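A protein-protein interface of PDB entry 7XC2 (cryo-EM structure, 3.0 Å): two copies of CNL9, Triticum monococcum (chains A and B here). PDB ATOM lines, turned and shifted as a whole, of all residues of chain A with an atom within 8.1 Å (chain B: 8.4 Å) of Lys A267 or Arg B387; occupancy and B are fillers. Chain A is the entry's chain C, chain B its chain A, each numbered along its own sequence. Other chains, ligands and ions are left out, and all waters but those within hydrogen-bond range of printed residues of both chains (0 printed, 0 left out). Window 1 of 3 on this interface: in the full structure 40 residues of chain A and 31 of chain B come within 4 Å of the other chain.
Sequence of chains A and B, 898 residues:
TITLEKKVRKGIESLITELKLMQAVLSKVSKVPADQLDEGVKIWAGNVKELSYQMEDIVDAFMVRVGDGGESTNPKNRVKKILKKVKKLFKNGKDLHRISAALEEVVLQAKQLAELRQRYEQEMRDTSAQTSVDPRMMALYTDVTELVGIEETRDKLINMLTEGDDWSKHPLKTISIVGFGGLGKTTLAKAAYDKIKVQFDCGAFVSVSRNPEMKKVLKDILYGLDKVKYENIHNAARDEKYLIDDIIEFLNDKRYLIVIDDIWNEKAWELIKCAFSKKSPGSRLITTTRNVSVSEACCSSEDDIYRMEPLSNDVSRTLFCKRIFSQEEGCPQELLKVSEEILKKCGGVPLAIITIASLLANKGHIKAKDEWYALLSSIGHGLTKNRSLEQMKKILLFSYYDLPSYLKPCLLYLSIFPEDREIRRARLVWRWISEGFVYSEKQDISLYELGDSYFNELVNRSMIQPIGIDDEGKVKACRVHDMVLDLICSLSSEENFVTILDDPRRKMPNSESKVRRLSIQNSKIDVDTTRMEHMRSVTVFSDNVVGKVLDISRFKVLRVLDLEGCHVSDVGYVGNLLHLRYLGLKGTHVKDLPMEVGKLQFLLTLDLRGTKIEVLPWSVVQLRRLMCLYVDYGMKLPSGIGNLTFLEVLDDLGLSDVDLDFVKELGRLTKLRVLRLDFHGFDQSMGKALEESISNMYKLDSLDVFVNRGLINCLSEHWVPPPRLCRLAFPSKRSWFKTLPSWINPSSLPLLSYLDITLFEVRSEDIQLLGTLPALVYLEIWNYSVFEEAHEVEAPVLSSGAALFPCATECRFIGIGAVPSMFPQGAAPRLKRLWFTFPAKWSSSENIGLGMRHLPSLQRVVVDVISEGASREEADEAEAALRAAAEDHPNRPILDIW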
ATOM      1  N   PRO A 212     -17.380   5.906  -4.543  1.00  0.00           N
ATOM      2  CA  PRO A 212     -16.263   6.072  -5.467  1.00  0.00           C
ATOM      3  C   PRO A 212     -14.958   6.425  -4.771  1.00  0.00           C
ATOM      4  O   PRO A 212     -14.926   6.905  -3.639  1.00  0.00           O
ATOM      5  CB  PRO A 212     -16.735   7.237  -6.339  1.00  0.00           C
ATOM      6  CG  PRO A 212     -17.521   8.061  -5.407  1.00  0.00           C
ATOM      7  CD  PRO A 212     -18.172   7.136  -4.423  1.00  0.00           C
ATOM      8  N   MET A 214     -11.915   8.925  -5.674  1.00  0.00           N
ATOM      9  CA  MET A 214     -11.727  10.032  -6.597  1.00  0.00           C
ATOM     10  C   MET A 214     -10.483   9.860  -7.451  1.00  0.00           C
ATOM     11  O   MET A 214     -10.477  10.257  -8.622  1.00  0.00           O
ATOM     12  CB  MET A 214     -11.679  11.334  -5.818  1.00  0.00           C
ATOM     13  CG  MET A 214     -13.024  11.720  -5.259  1.00  0.00           C
ATOM     14  SD  MET A 214     -14.200  12.095  -6.568  1.00  0.00           S
ATOM     15  CE  MET A 214     -15.290  10.693  -6.446  1.00  0.00           C
ATOM     16  N   ILE A 263     -23.853   9.296 -11.160  1.00  0.00           N
ATOM     17  CA  ILE A 263     -23.508  10.072  -9.975  1.00  0.00           C
ATOM     18  C   ILE A 263     -24.571   9.836  -8.917  1.00  0.00           C
ATOM     19  O   ILE A 263     -25.768   9.896  -9.206  1.00  0.00           O
ATOM     20  CB  ILE A 263     -23.393  11.562 -10.305  1.00  0.00           C
ATOM     21  CG1 ILE A 263     -22.554  11.766 -11.550  1.00  0.00           C
ATOM     22  CG2 ILE A 263     -22.747  12.288  -9.169  1.00  0.00           C
ATOM     23  CD1 ILE A 263     -22.291  13.200 -11.840  1.00  0.00           C
ATOM     24  N   TRP A 264     -24.142   9.574  -7.684  1.00  0.00           N
ATOM     25  CA  TRP A 264     -25.079   9.187  -6.644  1.00  0.00           C
ATOM     26  C   TRP A 264     -25.234  10.197  -5.522  1.00  0.00           C
ATOM     27  O   TRP A 264     -26.199  10.094  -4.764  1.00  0.00           O
ATOM     28  CB  TRP A 264     -24.679   7.837  -6.042  1.00  0.00           C
ATOM     29  CG  TRP A 264     -25.066   6.697  -6.903  1.00  0.00           C
ATOM     30  CD1 TRP A 264     -24.379   6.213  -7.960  1.00  0.00           C
ATOM     31  CD2 TRP A 264     -26.243   5.900  -6.792  1.00  0.00           C
ATOM     32  NE1 TRP A 264     -25.046   5.162  -8.521  1.00  0.00           N
ATOM     33  CE2 TRP A 264     -26.198   4.949  -7.818  1.00  0.00           C
ATOM     34  CE3 TRP A 264     -27.330   5.897  -5.923  1.00  0.00           C
ATOM     35  CZ2 TRP A 264     -27.190   4.007  -7.997  1.00  0.00           C
ATOM     36  CZ3 TRP A 264     -28.311   4.963  -6.104  1.00  0.00           C
ATOM     37  CH2 TRP A 264     -28.238   4.030  -7.131  1.00  0.00           C
ATOM     38  N   ASN A 265     -24.333  11.161  -5.386  1.00  0.00           N
ATOM     39  CA  ASN A 265     -24.545  12.235  -4.424  1.00  0.00           C
ATOM     40  C   ASN A 265     -23.744  13.452  -4.859  1.00  0.00           C
ATOM     41  O   ASN A 265     -23.249  13.525  -5.987  1.00  0.00           O
ATOM     42  CB  ASN A 265     -24.183  11.806  -3.002  1.00  0.00           C
ATOM     43  CG  ASN A 265     -22.729  11.484  -2.849  1.00  0.00           C
ATOM     44  OD1 ASN A 265     -21.980  11.466  -3.817  1.00  0.00           O
ATOM     45  ND2 ASN A 265     -22.309  11.254  -1.617  1.00  0.00           N
ATOM     46  N   GLU A 266     -23.596  14.401  -3.946  1.00  0.00           N
ATOM     47  CA  GLU A 266     -23.182  15.754  -4.277  1.00  0.00           C
ATOM     48  C   GLU A 266     -21.683  15.980  -4.159  1.00  0.00           C
ATOM     49  O   GLU A 266     -21.109  16.714  -4.969  1.00  0.00           O
ATOM     50  CB  GLU A 266     -23.914  16.734  -3.370  1.00  0.00           C
ATOM     51  CG  GLU A 266     -23.672  18.157  -3.721  1.00  0.00           C
ATOM     52  CD  GLU A 266     -24.271  18.501  -5.048  1.00  0.00           C
ATOM     53  OE1 GLU A 266     -25.260  17.843  -5.427  1.00  0.00           O
ATOM     54  OE2 GLU A 266     -23.752  19.420  -5.714  1.00  0.00           O
ATOM     55  N   LYS A 267     -21.041  15.386  -3.154  1.00  0.00           N
ATOM     56  CA  LYS A 267     -19.620  15.627  -2.937  1.00  0.00           C
ATOM     57  C   LYS A 267     -18.799  15.247  -4.156  1.00  0.00           C
ATOM     58  O   LYS A 267     -17.828  15.932  -4.503  1.00  0.00           O
ATOM     59  CB  LYS A 267     -19.136  14.843  -1.726  1.00  0.00           C
ATOM     60  CG  LYS A 267     -19.952  15.049  -0.484  1.00  0.00           C
ATOM     61  CD  LYS A 267     -19.343  14.278   0.669  1.00  0.00           C
ATOM     62  CE  LYS A 267     -20.099  14.517   1.962  1.00  0.00           C
ATOM     63  NZ  LYS A 267     -21.497  14.018   1.884  1.00  0.00           N
ATOM     64  N   ALA A 268     -19.164  14.148  -4.811  1.00  0.00           N
ATOM     65  CA  ALA A 268     -18.417  13.699  -5.976  1.00  0.00           C
ATOM     66  C   ALA A 268     -18.395  14.772  -7.050  1.00  0.00           C
ATOM     67  O   ALA A 268     -17.333  15.116  -7.579  1.00  0.00           O
ATOM     68  CB  ALA A 268     -19.023  12.408  -6.512  1.00  0.00           C
ATOM     69  N   TRP A 269     -19.562  15.311  -7.387  1.00  0.00           N
ATOM     70  CA  TRP A 269     -19.603  16.357  -8.395  1.00  0.00           C
ATOM     71  C   TRP A 269     -18.884  17.601  -7.914  1.00  0.00           C
ATOM     72  O   TRP A 269     -18.193  18.265  -8.691  1.00  0.00           O
ATOM     73  CB  TRP A 269     -21.039  16.696  -8.756  1.00  0.00           C
ATOM     74  CG  TRP A 269     -21.096  17.802  -9.718  1.00  0.00           C
ATOM     75  CD1 TRP A 269     -21.533  19.059  -9.487  1.00  0.00           C
ATOM     76  CD2 TRP A 269     -20.666  17.766 -11.074  1.00  0.00           C
ATOM     77  NE1 TRP A 269     -21.416  19.815 -10.619  1.00  0.00           N
ATOM     78  CE2 TRP A 269     -20.884  19.038 -11.611  1.00  0.00           C
ATOM     79  CE3 TRP A 269     -20.123  16.776 -11.890  1.00  0.00           C
ATOM     80  CZ2 TRP A 269     -20.581  19.348 -12.921  1.00  0.00           C
ATOM     81  CZ3 TRP A 269     -19.822  17.087 -13.185  1.00  0.00           C
ATOM     82  CH2 TRP A 269     -20.052  18.359 -13.692  1.00  0.00           C
ATOM     83  N   GLU A 270     -19.036  17.931  -6.636  1.00  0.00           N
ATOM     84  CA  GLU A 270     -18.373  19.107  -6.094  1.00  0.00           C
ATOM     85  C   GLU A 270     -16.868  19.030  -6.277  1.00  0.00           C
ATOM     86  O   GLU A 270     -16.216  20.055  -6.488  1.00  0.00           O
ATOM     87  CB  GLU A 270     -18.722  19.249  -4.619  1.00  0.00           C
ATOM     88  CG  GLU A 270     -18.290  20.541  -3.997  1.00  0.00           C
ATOM     89  CD  GLU A 270     -18.769  20.669  -2.568  1.00  0.00           C
ATOM     90  OE1 GLU A 270     -19.109  19.635  -1.959  1.00  0.00           O
ATOM     91  OE2 GLU A 270     -18.807  21.807  -2.052  1.00  0.00           O
ATOM     92  N   LEU A 271     -16.301  17.829  -6.207  1.00  0.00           N
ATOM     93  CA  LEU A 271     -14.859  17.706  -6.394  1.00  0.00           C
ATOM     94  C   LEU A 271     -14.482  17.655  -7.867  1.00  0.00           C
ATOM     95  O   LEU A 271     -13.527  18.312  -8.288  1.00  0.00           O
ATOM     96  CB  LEU A 271     -14.331  16.470  -5.675  1.00  0.00           C
ATOM     97  CG  LEU A 271     -12.808  16.391  -5.586  1.00  0.00           C
ATOM     98  CD1 LEU A 271     -12.416  15.778  -4.274  1.00  0.00           C
ATOM     99  CD2 LEU A 271     -12.221  15.579  -6.718  1.00  0.00           C
ATOM    100  N   ILE A 272     -15.202  16.865  -8.669  1.00  0.00           N
ATOM    101  CA  ILE A 272     -14.863  16.739 -10.086  1.00  0.00           C
ATOM    102  C   ILE A 272     -15.065  18.030 -10.852  1.00  0.00           C
ATOM    103  O   ILE A 272     -14.399  18.249 -11.868  1.00  0.00           O
ATOM    104  CB  ILE A 272     -15.694  15.616 -10.739  1.00  0.00           C
ATOM    105  CG1 ILE A 272     -15.469  14.305 -10.001  1.00  0.00           C
ATOM    106  CG2 ILE A 272     -15.330  15.436 -12.184  1.00  0.00           C
ATOM    107  CD1 ILE A 272     -16.323  13.186 -10.508  1.00  0.00           C
ATOM    108  N   LYS A 273     -15.926  18.917 -10.373  1.00  0.00           N
ATOM    109  CA  LYS A 273     -16.178  20.169 -11.061  1.00  0.00           C
ATOM    110  C   LYS A 273     -14.941  21.050 -11.134  1.00  0.00           C
ATOM    111  O   LYS A 273     -14.878  21.940 -11.985  1.00  0.00           O
ATOM    112  CB  LYS A 273     -17.314  20.882 -10.339  1.00  0.00           C
ATOM    113  CG  LYS A 273     -17.631  22.270 -10.793  1.00  0.00           C
ATOM    114  CD  LYS A 273     -18.578  22.905  -9.800  1.00  0.00           C
ATOM    115  CE  LYS A 273     -19.274  24.109 -10.389  1.00  0.00           C
ATOM    116  NZ  LYS A 273     -20.398  24.553  -9.527  1.00  0.00           N
ATOM    117  N   VAL A 294     -29.195  16.195  -7.260  1.00  0.00           N
ATOM    118  CA  VAL A 294     -27.888  16.175  -7.901  1.00  0.00           C
ATOM    119  C   VAL A 294     -27.962  16.813  -9.277  1.00  0.00           C
ATOM    120  O   VAL A 294     -27.069  17.574  -9.666  1.00  0.00           O
ATOM    121  CB  VAL A 294     -27.364  14.735  -7.976  1.00  0.00           C
ATOM    122  CG1 VAL A 294     -26.071  14.684  -8.735  1.00  0.00           C
ATOM    123  CG2 VAL A 294     -27.181  14.173  -6.592  1.00  0.00           C
ATOM    124  N   ALA A 297     -28.112  20.462  -8.968  1.00  0.00           N
ATOM    125  CA  ALA A 297     -26.814  21.012  -8.605  1.00  0.00           C
ATOM    126  C   ALA A 297     -25.842  21.024  -9.772  1.00  0.00           C
ATOM    127  O   ALA A 297     -24.930  21.854  -9.799  1.00  0.00           O
ATOM    128  CB  ALA A 297     -26.219  20.220  -7.450  1.00  0.00           C
ATOM    129  N   SER B 132     -12.272  10.755   2.704  1.00  0.00           N
ATOM    130  CA  SER B 132     -12.648  11.984   2.028  1.00  0.00           C
ATOM    131  C   SER B 132     -11.415  12.847   1.791  1.00  0.00           C
ATOM    132  O   SER B 132     -10.319  12.559   2.268  1.00  0.00           O
ATOM    133  CB  SER B 132     -13.696  12.759   2.822  1.00  0.00           C
ATOM    134  OG  SER B 132     -13.165  13.180   4.065  1.00  0.00           O
ATOM    135  N   VAL B 133     -11.613  13.914   1.036  1.00  0.00           N
ATOM    136  CA  VAL B 133     -10.551  14.828   0.684  1.00  0.00           C
ATOM    137  C   VAL B 133     -10.655  16.048   1.587  1.00  0.00           C
ATOM    138  O   VAL B 133     -11.714  16.357   2.133  1.00  0.00           O
ATOM    139  CB  VAL B 133     -10.641  15.204  -0.811  1.00  0.00           C
ATOM    140  CG1 VAL B 133      -9.448  16.009  -1.255  1.00  0.00           C
ATOM    141  CG2 VAL B 133     -10.765  13.952  -1.638  1.00  0.00           C
ATOM    142  N   PRO B 135     -11.403  19.488   2.821  1.00  0.00           N
ATOM    143  CA  PRO B 135     -12.340  20.487   2.289  1.00  0.00           C
ATOM    144  C   PRO B 135     -11.678  21.767   1.845  1.00  0.00           C
ATOM    145  O   PRO B 135     -12.289  22.529   1.090  1.00  0.00           O
ATOM    146  CB  PRO B 135     -13.289  20.740   3.462  1.00  0.00           C
ATOM    147  CG  PRO B 135     -13.166  19.560   4.307  1.00  0.00           C
ATOM    148  CD  PRO B 135     -11.759  19.093   4.188  1.00  0.00           C
ATOM    149  N   MET B 138     -10.629  22.601  -2.490  1.00  0.00           N
ATOM    150  CA  MET B 138     -11.388  23.239  -3.555  1.00  0.00           C
ATOM    151  C   MET B 138     -11.129  24.732  -3.630  1.00  0.00           C
ATOM    152  O   MET B 138     -11.222  25.313  -4.716  1.00  0.00           O
ATOM    153  CB  MET B 138     -12.877  22.983  -3.365  1.00  0.00           C
ATOM    154  CG  MET B 138     -13.344  21.656  -3.914  1.00  0.00           C
ATOM    155  SD  MET B 138     -12.874  20.257  -2.892  1.00  0.00           S
ATOM    156  CE  MET B 138     -14.143  20.334  -1.641  1.00  0.00           C
ATOM    157  N   THR B 355     -19.876  31.778   4.021  1.00  0.00           N
ATOM    158  CA  THR B 355     -20.836  30.719   4.321  1.00  0.00           C
ATOM    159  C   THR B 355     -22.205  31.285   4.665  1.00  0.00           C
ATOM    160  O   THR B 355     -23.225  30.784   4.180  1.00  0.00           O
ATOM    161  CB  THR B 355     -20.334  29.839   5.455  1.00  0.00           C
ATOM    162  OG1 THR B 355     -20.040  30.655   6.589  1.00  0.00           O
ATOM    163  CG2 THR B 355     -19.088  29.104   5.032  1.00  0.00           C
ATOM    164  N   SER B 358     -23.937  32.537   1.547  1.00  0.00           N
ATOM    165  CA  SER B 358     -24.534  31.461   0.761  1.00  0.00           C
ATOM    166  C   SER B 358     -25.780  30.920   1.432  1.00  0.00           C
ATOM    167  O   SER B 358     -26.737  30.544   0.749  1.00  0.00           O
ATOM    168  CB  SER B 358     -23.533  30.334   0.541  1.00  0.00           C
ATOM    169  OG  SER B 358     -23.720  29.324   1.511  1.00  0.00           O
ATOM    170  N   LEU B 359     -25.796  30.889   2.760  1.00  0.00           N
ATOM    171  CA  LEU B 359     -26.970  30.416   3.483  1.00  0.00           C
ATOM    172  C   LEU B 359     -28.169  31.325   3.253  1.00  0.00           C
ATOM    173  O   LEU B 359     -29.284  30.845   3.022  1.00  0.00           O
ATOM    174  CB  LEU B 359     -26.658  30.322   4.973  1.00  0.00           C
ATOM    175  CG  LEU B 359     -27.663  29.583   5.843  1.00  0.00           C
ATOM    176  CD1 LEU B 359     -27.745  28.161   5.381  1.00  0.00           C
ATOM    177  CD2 LEU B 359     -27.239  29.632   7.293  1.00  0.00           C
ATOM    178  N   ASN B 386     -27.036  21.803   5.809  1.00  0.00           N
ATOM    179  CA  ASN B 386     -26.448  22.475   4.658  1.00  0.00           C
ATOM    180  C   ASN B 386     -24.991  22.075   4.487  1.00  0.00           C
ATOM    181  O   ASN B 386     -24.307  21.777   5.460  1.00  0.00           O
ATOM    182  CB  ASN B 386     -26.563  23.988   4.805  1.00  0.00           C
ATOM    183  CG  ASN B 386     -26.144  24.718   3.557  1.00  0.00           C
ATOM    184  OD1 ASN B 386     -25.975  24.110   2.505  1.00  0.00           O
ATOM    185  ND2 ASN B 386     -25.979  26.027   3.662  1.00  0.00           N
ATOM    186  N   ARG B 387     -24.516  22.083   3.241  1.00  0.00           N
ATOM    187  CA  ARG B 387     -23.165  21.616   2.951  1.00  0.00           C
ATOM    188  C   ARG B 387     -22.111  22.618   3.402  1.00  0.00           C
ATOM    189  O   ARG B 387     -21.137  22.246   4.066  1.00  0.00           O
ATOM    190  CB  ARG B 387     -23.018  21.335   1.458  1.00  0.00           C
ATOM    191  CG  ARG B 387     -23.641  20.030   1.011  1.00  0.00           C
ATOM    192  CD  ARG B 387     -22.956  19.492  -0.230  1.00  0.00           C
ATOM    193  NE  ARG B 387     -21.504  19.548  -0.116  1.00  0.00           N
ATOM    194  CZ  ARG B 387     -20.784  18.730   0.644  1.00  0.00           C
ATOM    195  NH1 ARG B 387     -21.381  17.794   1.364  1.00  0.00           N
ATOM    196  NH2 ARG B 387     -19.466  18.850   0.690  1.00  0.00           N
ATOM    197  N   SER B 388     -22.278  23.889   3.039  1.00  0.00           N
ATOM    198  CA  SER B 388     -21.278  24.884   3.396  1.00  0.00           C
ATOM    199  C   SER B 388     -21.096  24.978   4.903  1.00  0.00           C
ATOM    200  O   SER B 388     -19.969  25.134   5.386  1.00  0.00           O
ATOM    201  CB  SER B 388     -21.670  26.242   2.828  1.00  0.00           C
ATOM    202  OG  SER B 388     -22.217  26.097   1.534  1.00  0.00           O
ATOM    203  N   LEU B 389     -22.183  24.861   5.657  1.00  0.00           N
ATOM    204  CA  LEU B 389     -22.082  24.960   7.104  1.00  0.00           C
ATOM    205  C   LEU B 389     -21.318  23.776   7.683  1.00  0.00           C
ATOM    206  O   LEU B 389     -20.478  23.944   8.576  1.00  0.00           O
ATOM    207  CB  LEU B 389     -23.481  25.060   7.692  1.00  0.00           C
ATOM    208  CG  LEU B 389     -23.615  25.401   9.162  1.00  0.00           C
ATOM    209  CD1 LEU B 389     -23.070  26.782   9.409  1.00  0.00           C
ATOM    210  CD2 LEU B 389     -25.072  25.328   9.550  1.00  0.00           C
ATOM    211  N   GLU B 390     -21.586  22.573   7.173  1.00  0.00           N
ATOM    212  CA  GLU B 390     -20.821  21.406   7.593  1.00  0.00           C
ATOM    213  C   GLU B 390     -19.344  21.573   7.275  1.00  0.00           C
ATOM    214  O   GLU B 390     -18.484  21.215   8.084  1.00  0.00           O
ATOM    215  CB  GLU B 390     -21.363  20.156   6.914  1.00  0.00           C
ATOM    216  CG  GLU B 390     -22.704  19.698   7.436  1.00  0.00           C
ATOM    217  CD  GLU B 390     -23.438  18.814   6.448  1.00  0.00           C
ATOM    218  OE1 GLU B 390     -23.404  19.111   5.235  1.00  0.00           O
ATOM    219  OE2 GLU B 390     -24.043  17.812   6.881  1.00  0.00           O
ATOM    220  N   GLN B 391     -19.031  22.113   6.099  1.00  0.00           N
ATOM    221  CA  GLN B 391     -17.634  22.316   5.742  1.00  0.00           C
ATOM    222  C   GLN B 391     -16.960  23.302   6.680  1.00  0.00           C
ATOM    223  O   GLN B 391     -15.828  23.077   7.117  1.00  0.00           O
ATOM    224  CB  GLN B 391     -17.523  22.801   4.305  1.00  0.00           C
ATOM    225  CG  GLN B 391     -17.721  21.723   3.282  1.00  0.00           C
ATOM    226  CD  GLN B 391     -17.445  22.220   1.890  1.00  0.00           C
ATOM    227  OE1 GLN B 391     -16.729  23.201   1.703  1.00  0.00           O
ATOM    228  NE2 GLN B 391     -18.018  21.552   0.900  1.00  0.00           N
ATOM    229  N   MET B 392     -17.632  24.409   6.993  1.00  0.00           N
ATOM    230  CA  MET B 392     -17.029  25.389   7.888  1.00  0.00           C
ATOM    231  C   MET B 392     -16.777  24.797   9.263  1.00  0.00           C
ATOM    232  O   MET B 392     -15.718  25.015   9.860  1.00  0.00           O
ATOM    233  CB  MET B 392     -17.914  26.621   8.009  1.00  0.00           C
ATOM    234  CG  MET B 392     -17.288  27.703   8.845  1.00  0.00           C
ATOM    235  SD  MET B 392     -18.335  29.142   9.066  1.00  0.00           S
ATOM    236  CE  MET B 392     -19.483  28.510  10.273  1.00  0.00           C
ATOM    237  N   LYS B 393     -17.746  24.052   9.788  1.00  0.00           N
ATOM    238  CA  LYS B 393     -17.561  23.428  11.090  1.00  0.00           C
ATOM    239  C   LYS B 393     -16.395  22.448  11.065  1.00  0.00           C
ATOM    240  O   LYS B 393     -15.540  22.451  11.961  1.00  0.00           O
ATOM    241  CB  LYS B 393     -18.850  22.734  11.510  1.00  0.00           C
ATOM    242  CG  LYS B 393     -18.684  21.718  12.602  1.00  0.00           C
ATOM    243  CD  LYS B 393     -20.010  21.068  12.922  1.00  0.00           C
ATOM    244  CE  LYS B 393     -19.853  19.971  13.950  1.00  0.00           C
ATOM    245  NZ  LYS B 393     -21.159  19.365  14.311  1.00  0.00           N
ATOM    246  N   LYS B 394     -16.339  21.606  10.037  1.00  0.00           N
ATOM    247  CA  LYS B 394     -15.261  20.636   9.936  1.00  0.00           C
ATOM    248  C   LYS B 394     -13.907  21.320   9.833  1.00  0.00           C
ATOM    249  O   LYS B 394     -12.913  20.824  10.370  1.00  0.00           O
ATOM    250  CB  LYS B 394     -15.500  19.733   8.733  1.00  0.00           C
ATOM    251  CG  LYS B 394     -14.386  18.775   8.436  1.00  0.00           C
ATOM    252  CD  LYS B 394     -14.743  17.901   7.258  1.00  0.00           C
ATOM    253  CE  LYS B 394     -13.709  16.816   7.053  1.00  0.00           C
ATOM    254  NZ  LYS B 394     -14.107  15.869   5.979  1.00  0.00           N
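Lys A267 touches one residue of chain B.
Of chain A, only Glu A266, Lys A267 and Glu A270 come within 4 Å of Arg B387.
No residue of chain B comes within 4 Å of Ala A268.
Printed residues of chain B within 4 Å of Leu A271: Val B133.
Printed residues of chain A within 4 Å of Gln B391: Glu A270.
Of the printed residues of chain A, Val B133 touches Leu A271.
Printed residues of chain B within 4 Å of Glu A270: Arg B387 and Gln B391.
Printed residues of chain B within 4 Å of Glu A266: Arg B387.
Pro B135 touches none of the printed residues of chain A.
Pro A212 touches none of the printed residues of chain B.
The nearest printed residue of chain B that does not touch Glu A266 is Gln B391 (8.1 Å).
The side-chain amide nitrogen (NE2) of Gln B391 lies close to the guanidinium group (NH2) of Arg B387, 3.1 Å away.
Of the 15 printed residues of chain A, 4 touch a printed residue of chain B.
Hydrophobic or aromatic side chains of chain A that line the printed part of chain B: Leu A271.
Of the 16 printed residues of chain B, 3 touch a printed residue of chain A.
Among the printed residues, 5 pairs touch across the chains.
Among the printed residues, Asp or Glu carboxylates within 4 Å of a Lys or Arg side-chain nitrogen of the other chain: Glu A270 with Arg B387 (2.8 Å).
No position is printed for both chains.
Among the printed residues, pairs that only touch across the chains: Lys A267 with Arg B387 (3.6 Å), Leu A271 with Val B133 (3.6 Å) and Glu A266 with Arg B387 (3.8 Å).
NH2 of Arg B387 lies within salt-bridge range of OE1 of Glu A270 (2.8 Å).
NE2 of Gln B391 is in hydrogen-bond range of OE2 of Glu A270 (3.1 Å).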
